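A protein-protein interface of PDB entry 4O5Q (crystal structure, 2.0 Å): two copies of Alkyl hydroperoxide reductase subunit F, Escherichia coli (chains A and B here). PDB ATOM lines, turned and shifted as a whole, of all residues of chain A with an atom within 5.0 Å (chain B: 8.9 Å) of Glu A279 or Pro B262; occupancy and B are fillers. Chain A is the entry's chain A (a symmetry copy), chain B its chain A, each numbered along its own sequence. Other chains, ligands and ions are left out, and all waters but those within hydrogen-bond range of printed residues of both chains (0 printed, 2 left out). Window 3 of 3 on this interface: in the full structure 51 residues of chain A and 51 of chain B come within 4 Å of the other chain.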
ATOM      1  N   VAL A 275     -35.711  18.826 -33.910  1.00  0.00           N
ATOM      2  CA  VAL A 275     -35.582  17.423 -33.510  1.00  0.00           C
ATOM      3  C   VAL A 275     -35.046  17.329 -32.053  1.00  0.00           C
ATOM      4  O   VAL A 275     -35.557  16.573 -31.238  1.00  0.00           O
ATOM      5  CB  VAL A 275     -34.644  16.676 -34.483  1.00  0.00           C
ATOM      6  CG1 VAL A 275     -34.204  15.279 -33.930  1.00  0.00           C
ATOM      7  CG2 VAL A 275     -35.335  16.506 -35.880  1.00  0.00           C
ATOM      8  N   HIS A 276     -34.046  18.133 -31.724  1.00  0.00           N
ATOM      9  CA  HIS A 276     -33.460  18.062 -30.390  1.00  0.00           C
ATOM     10  C   HIS A 276     -34.473  18.484 -29.332  1.00  0.00           C
ATOM     11  O   HIS A 276     -34.635  17.806 -28.300  1.00  0.00           O
ATOM     12  CB  HIS A 276     -32.202  18.916 -30.313  1.00  0.00           C
ATOM     13  CG  HIS A 276     -31.250  18.505 -29.236  1.00  0.00           C
ATOM     14  ND1 HIS A 276     -29.993  19.041 -29.134  1.00  0.00           N
ATOM     15  CD2 HIS A 276     -31.335  17.552 -28.267  1.00  0.00           C
ATOM     16  CE1 HIS A 276     -29.351  18.465 -28.125  1.00  0.00           C
ATOM     17  NE2 HIS A 276     -30.141  17.572 -27.585  1.00  0.00           N
ATOM     18  N   VAL A 277     -35.170  19.598 -29.585  1.00  0.00           N
ATOM     19  CA  VAL A 277     -36.235  20.058 -28.716  1.00  0.00           C
ATOM     20  C   VAL A 277     -37.326  19.008 -28.546  1.00  0.00           C
ATOM     21  O   VAL A 277     -37.765  18.703 -27.421  1.00  0.00           O
ATOM     22  CB  VAL A 277     -36.883  21.380 -29.270  1.00  0.00           C
ATOM     23  CG1 VAL A 277     -38.224  21.645 -28.623  1.00  0.00           C
ATOM     24  CG2 VAL A 277     -35.933  22.560 -29.075  1.00  0.00           C
ATOM     25  N   ASP A 278     -37.755  18.429 -29.655  1.00  0.00           N
ATOM     26  CA  ASP A 278     -38.880  17.504 -29.607  1.00  0.00           C
ATOM     27  C   ASP A 278     -38.540  16.177 -28.880  1.00  0.00           C
ATOM     28  O   ASP A 278     -39.443  15.424 -28.504  1.00  0.00           O
ATOM     29  CB  ASP A 278     -39.369  17.211 -31.030  1.00  0.00           C
ATOM     30  CG  ASP A 278     -40.287  18.307 -31.586  1.00  0.00           C
ATOM     31  OD1 ASP A 278     -40.799  19.143 -30.812  1.00  0.00           O
ATOM     32  OD2 ASP A 278     -40.517  18.302 -32.810  1.00  0.00           O
ATOM     33  N   GLU A 279     -37.255  15.876 -28.700  1.00  0.00           N
ATOM     34  CA  GLU A 279     -36.860  14.675 -27.955  1.00  0.00           C
ATOM     35  C   GLU A 279     -37.358  14.757 -26.525  1.00  0.00           C
ATOM     36  O   GLU A 279     -37.578  13.746 -25.890  1.00  0.00           O
ATOM     37  CB  GLU A 279     -35.361  14.477 -27.919  1.00  0.00           C
ATOM     38  CG  GLU A 279     -34.731  14.116 -29.230  1.00  0.00           C
ATOM     39  CD  GLU A 279     -33.858  12.896 -29.094  1.00  0.00           C
ATOM     40  OE1 GLU A 279     -34.071  11.938 -29.874  1.00  0.00           O
ATOM     41  OE2 GLU A 279     -32.979  12.895 -28.195  1.00  0.00           O
ATOM     42  N   TYR A 280     -37.565  15.965 -26.026  1.00  0.00           N
ATOM     43  CA  TYR A 280     -37.948  16.145 -24.622  1.00  0.00           C
ATOM     44  C   TYR A 280     -39.374  16.614 -24.388  1.00  0.00           C
ATOM     45  O   TYR A 280     -39.738  16.982 -23.261  1.00  0.00           O
ATOM     46  CB  TYR A 280     -36.941  17.104 -23.971  1.00  0.00           C
ATOM     47  CG  TYR A 280     -35.553  16.534 -24.032  1.00  0.00           C
ATOM     48  CD1 TYR A 280     -35.187  15.489 -23.196  1.00  0.00           C
ATOM     49  CD2 TYR A 280     -34.630  16.986 -24.959  1.00  0.00           C
ATOM     50  CE1 TYR A 280     -33.926  14.930 -23.263  1.00  0.00           C
ATOM     51  CE2 TYR A 280     -33.354  16.441 -25.033  1.00  0.00           C
ATOM     52  CZ  TYR A 280     -33.008  15.415 -24.165  1.00  0.00           C
ATOM     53  OH  TYR A 280     -31.750  14.848 -24.213  1.00  0.00           O
ATOM     54  N   ASP A 281     -40.190  16.630 -25.430  1.00  0.00           N
ATOM     55  CA  ASP A 281     -41.629  16.910 -25.248  1.00  0.00           C
ATOM     56  C   ASP A 281     -41.891  18.306 -24.635  1.00  0.00           C
ATOM     57  O   ASP A 281     -42.759  18.503 -23.795  1.00  0.00           O
ATOM     58  CB  ASP A 281     -42.300  15.831 -24.383  1.00  0.00           C
ATOM     59  CG  ASP A 281     -42.103  14.416 -24.932  1.00  0.00           C
ATOM     60  OD1 ASP A 281     -41.842  14.263 -26.149  1.00  0.00           O
ATOM     61  OD2 ASP A 281     -42.202  13.453 -24.135  1.00  0.00           O
ATOM     62  N   ASP B 254     -21.319   9.309 -23.882  1.00  0.00           N
ATOM     63  CA  ASP B 254     -22.599   9.910 -24.238  1.00  0.00           C
ATOM     64  C   ASP B 254     -22.788  11.413 -23.930  1.00  0.00           C
ATOM     65  O   ASP B 254     -22.697  11.857 -22.793  1.00  0.00           O
ATOM     66  CB  ASP B 254     -23.635   9.145 -23.444  1.00  0.00           C
ATOM     67  CG  ASP B 254     -25.003   9.533 -23.777  1.00  0.00           C
ATOM     68  OD1 ASP B 254     -25.291   9.566 -24.990  1.00  0.00           O
ATOM     69  OD2 ASP B 254     -25.785   9.794 -22.832  1.00  0.00           O
ATOM     70  N   ILE B 255     -23.086  12.191 -24.954  1.00  0.00           N
ATOM     71  CA  ILE B 255     -23.395  13.628 -24.764  1.00  0.00           C
ATOM     72  C   ILE B 255     -24.702  13.905 -25.488  1.00  0.00           C
ATOM     73  O   ILE B 255     -24.812  13.689 -26.706  1.00  0.00           O
ATOM     74  CB  ILE B 255     -22.272  14.479 -25.361  1.00  0.00           C
ATOM     75  CG1 ILE B 255     -20.940  14.189 -24.693  1.00  0.00           C
ATOM     76  CG2 ILE B 255     -22.603  15.974 -25.326  1.00  0.00           C
ATOM     77  CD1 ILE B 255     -19.791  14.766 -25.503  1.00  0.00           C
ATOM     78  N   GLU B 256     -25.699  14.344 -24.742  1.00  0.00           N
ATOM     79  CA  GLU B 256     -27.034  14.605 -25.294  1.00  0.00           C
ATOM     80  C   GLU B 256     -27.521  16.044 -25.206  1.00  0.00           C
ATOM     81  O   GLU B 256     -28.707  16.326 -25.474  1.00  0.00           O
ATOM     82  CB  GLU B 256     -28.036  13.679 -24.604  1.00  0.00           C
ATOM     83  CG  GLU B 256     -27.681  12.224 -24.931  1.00  0.00           C
ATOM     84  CD  GLU B 256     -28.623  11.226 -24.289  1.00  0.00           C
ATOM     85  OE1 GLU B 256     -28.266  10.670 -23.240  1.00  0.00           O
ATOM     86  OE2 GLU B 256     -29.706  10.988 -24.845  1.00  0.00           O
ATOM     87  N   ASN B 257     -26.623  16.950 -24.824  1.00  0.00           N
ATOM     88  CA  ASN B 257     -27.000  18.370 -24.726  1.00  0.00           C
ATOM     89  C   ASN B 257     -26.060  19.315 -25.472  1.00  0.00           C
ATOM     90  O   ASN B 257     -26.060  20.539 -25.198  1.00  0.00           O
ATOM     91  CB  ASN B 257     -27.140  18.780 -23.234  1.00  0.00           C
ATOM     92  CG  ASN B 257     -25.851  18.578 -22.463  1.00  0.00           C
ATOM     93  OD1 ASN B 257     -24.820  18.204 -23.032  1.00  0.00           O
ATOM     94  ND2 ASN B 257     -25.904  18.797 -21.161  1.00  0.00           N
ATOM     95  N   TYR B 258     -25.319  18.803 -26.472  1.00  0.00           N
ATOM     96  CA  TYR B 258     -24.644  19.702 -27.399  1.00  0.00           C
ATOM     97  C   TYR B 258     -25.696  20.143 -28.426  1.00  0.00           C
ATOM     98  O   TYR B 258     -26.048  19.395 -29.332  1.00  0.00           O
ATOM     99  CB  TYR B 258     -23.381  19.111 -28.083  1.00  0.00           C
ATOM    100  CG  TYR B 258     -22.576  20.203 -28.741  1.00  0.00           C
ATOM    101  CD1 TYR B 258     -21.782  21.050 -27.978  1.00  0.00           C
ATOM    102  CD2 TYR B 258     -22.653  20.444 -30.103  1.00  0.00           C
ATOM    103  CE1 TYR B 258     -21.063  22.046 -28.525  1.00  0.00           C
ATOM    104  CE2 TYR B 258     -21.920  21.478 -30.675  1.00  0.00           C
ATOM    105  CZ  TYR B 258     -21.138  22.269 -29.896  1.00  0.00           C
ATOM    106  OH  TYR B 258     -20.398  23.277 -30.421  1.00  0.00           O
ATOM    107  N   ILE B 259     -26.216  21.348 -28.216  1.00  0.00           N
ATOM    108  CA  ILE B 259     -27.413  21.802 -28.878  1.00  0.00           C
ATOM    109  C   ILE B 259     -27.342  21.619 -30.402  1.00  0.00           C
ATOM    110  O   ILE B 259     -26.393  22.021 -31.059  1.00  0.00           O
ATOM    111  CB  ILE B 259     -27.732  23.284 -28.486  1.00  0.00           C
ATOM    112  CG1 ILE B 259     -27.869  23.418 -26.956  1.00  0.00           C
ATOM    113  CG2 ILE B 259     -28.962  23.793 -29.234  1.00  0.00           C
ATOM    114  CD1 ILE B 259     -28.869  22.489 -26.282  1.00  0.00           C
ATOM    115  N   SER B 260     -28.400  20.996 -30.906  1.00  0.00           N
ATOM    116  CA  SER B 260     -28.618  20.577 -32.302  1.00  0.00           C
ATOM    117  C   SER B 260     -28.178  19.167 -32.578  1.00  0.00           C
ATOM    118  O   SER B 260     -28.532  18.609 -33.614  1.00  0.00           O
ATOM    119  CB  SER B 260     -28.091  21.573 -33.369  1.00  0.00           C
ATOM    120  OG  SER B 260     -26.722  21.438 -33.557  1.00  0.00           O
ATOM    121  N   VAL B 261     -27.500  18.547 -31.619  1.00  0.00           N
ATOM    122  CA  VAL B 261     -27.022  17.197 -31.808  1.00  0.00           C
ATOM    123  C   VAL B 261     -27.664  16.307 -30.751  1.00  0.00           C
ATOM    124  O   VAL B 261     -27.244  16.335 -29.585  1.00  0.00           O
ATOM    125  CB  VAL B 261     -25.485  17.144 -31.726  1.00  0.00           C
ATOM    126  CG1 VAL B 261     -24.969  15.686 -31.942  1.00  0.00           C
ATOM    127  CG2 VAL B 261     -24.866  18.074 -32.730  1.00  0.00           C
ATOM    128  N   PRO B 262     -28.683  15.520 -31.128  1.00  0.00           N
ATOM    129  CA  PRO B 262     -29.397  14.829 -30.039  1.00  0.00           C
ATOM    130  C   PRO B 262     -28.538  13.883 -29.223  1.00  0.00           C
ATOM    131  O   PRO B 262     -28.769  13.731 -28.018  1.00  0.00           O
ATOM    132  CB  PRO B 262     -30.505  14.037 -30.771  1.00  0.00           C
ATOM    133  CG  PRO B 262     -30.816  14.905 -32.009  1.00  0.00           C
ATOM    134  CD  PRO B 262     -29.423  15.448 -32.413  1.00  0.00           C
ATOM    135  N   LYS B 263     -27.557  13.274 -29.875  1.00  0.00           N
ATOM    136  CA  LYS B 263     -26.700  12.294 -29.211  1.00  0.00           C
ATOM    137  C   LYS B 263     -25.407  12.174 -29.955  1.00  0.00           C
ATOM    138  O   LYS B 263     -25.392  11.971 -31.168  1.00  0.00           O
ATOM    139  CB  LYS B 263     -27.378  10.928 -29.139  1.00  0.00           C
ATOM    140  CG  LYS B 263     -26.662   9.943 -28.203  1.00  0.00           C
ATOM    141  CD  LYS B 263     -27.562   8.756 -27.839  1.00  0.00           C
ATOM    142  CE  LYS B 263     -26.782   7.634 -27.148  1.00  0.00           C
ATOM    143  NZ  LYS B 263     -27.671   6.632 -26.485  1.00  0.00           N
ATOM    144  N   THR B 264     -24.298  12.352 -29.244  1.00  0.00           N
ATOM    145  CA  THR B 264     -23.015  12.101 -29.845  1.00  0.00           C
ATOM    146  C   THR B 264     -22.144  11.518 -28.771  1.00  0.00           C
ATOM    147  O   THR B 264     -22.619  11.214 -27.693  1.00  0.00           O
ATOM    148  CB  THR B 264     -22.398  13.369 -30.523  1.00  0.00           C
ATOM    149  OG1 THR B 264     -21.189  12.994 -31.161  1.00  0.00           O
ATOM    150  CG2 THR B 264     -22.088  14.479 -29.516  1.00  0.00           C
ATOM    151  N   GLU B 265     -20.864  11.346 -29.072  1.00  0.00           N
ATOM    152  CA  GLU B 265     -19.921  10.826 -28.121  1.00  0.00           C
ATOM    153  C   GLU B 265     -18.739  11.749 -28.055  1.00  0.00           C
ATOM    154  O   GLU B 265     -18.407  12.428 -29.019  1.00  0.00           O
ATOM    155  CB  GLU B 265     -19.453   9.432 -28.542  1.00  0.00           C
ATOM    156  CG  GLU B 265     -20.585   8.450 -28.630  1.00  0.00           C
ATOM    157  CD  GLU B 265     -20.154   7.159 -29.280  1.00  0.00           C
ATOM    158  OE1 GLU B 265     -20.334   6.096 -28.647  1.00  0.00           O
ATOM    159  OE2 GLU B 265     -19.634   7.213 -30.417  1.00  0.00           O
ATOM    160  N   LYS B 354     -33.669   8.370 -14.619  1.00  0.00           N
ATOM    161  CA  LYS B 354     -35.116   8.347 -14.406  1.00  0.00           C
ATOM    162  C   LYS B 354     -35.524   7.002 -13.856  1.00  0.00           C
ATOM    163  O   LYS B 354     -35.142   5.966 -14.401  1.00  0.00           O
ATOM    164  CB  LYS B 354     -35.867   8.577 -15.720  1.00  0.00           C
ATOM    165  CG  LYS B 354     -35.642   9.924 -16.341  1.00  0.00           C
ATOM    166  CD  LYS B 354     -36.163   9.976 -17.788  1.00  0.00           C
ATOM    167  CE  LYS B 354     -37.643  10.328 -17.837  1.00  0.00           C
ATOM    168  NZ  LYS B 354     -38.069  10.827 -19.194  1.00  0.00           N
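Of the printed residues of chain B, Glu A279 touches Pro B262 (3.7 Å). Of chain B, only Glu B256, Tyr B258, Ile B259, Ser B260, Val B261 and Pro B262 come within 4 Å of His A276. Tyr A280 touches just one residue of chain B: Glu B256. Printed residues of chain B within 4 Å of Val A275: Pro B262. Printed residues of chain A within 4 Å of Ser B260: His A276. Of the printed residues of chain A, Ile B259 touches His A276. Printed residues of chain A within 4 Å of Val B261: His A276 (3.3 Å). Ile B255 touches none of the printed residues of chain A. Lys B354 touches none of the printed residues of chain A. The nearest printed residue of chain B that does not touch Glu A279 is Glu B256 (5.1 Å). The nearest printed residue of chain A that does not touch Ser B260 is Val A275 (6.5 Å).
Of the 7 printed residues of chain A, 4 touch a printed residue of chain B. Printed residues of chain A that touch a printed residue of chain B: Val A275, His A276, Glu A279 and Tyr A280. Hydrophobic or aromatic side chains of chain A that line the printed part of chain B: Val A275, His A276 and Tyr A280. Of the 13 printed residues of chain B, 6 touch a printed residue of chain A. Printed residues of chain B that touch a printed residue of chain A: Glu B256, Tyr B258, Ile B259, Ser B260, Val B261 and Pro B262. Among the printed residues, no Asp or Glu carboxylate lies within 4 Å of a Lys or Arg side-chain nitrogen of the other chain.
OD2 of Asp B254 sits close to OE1 of Glu B256, 2.7 Å away.
Among the printed residues, pairs that only touch across the chains: His A276 with Val B261, Tyr A280 with Glu B256, His A276 with Tyr B258, Glu A279 with Pro B262, His A276 with Pro B262, His A276 with Ile B259 and Val A275 with Pro B262.
The backbone carbonyl oxygen (O) of Glu B256 sits at hydrogen-bond distance from a ring nitrogen (NE2) of His A276, at 2.8 Å. The backbone NH of Ser B260 is in hydrogen-bond range of a ring nitrogen (ND1) of His A276, 3.1 Å away.
No position is printed for both chains.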
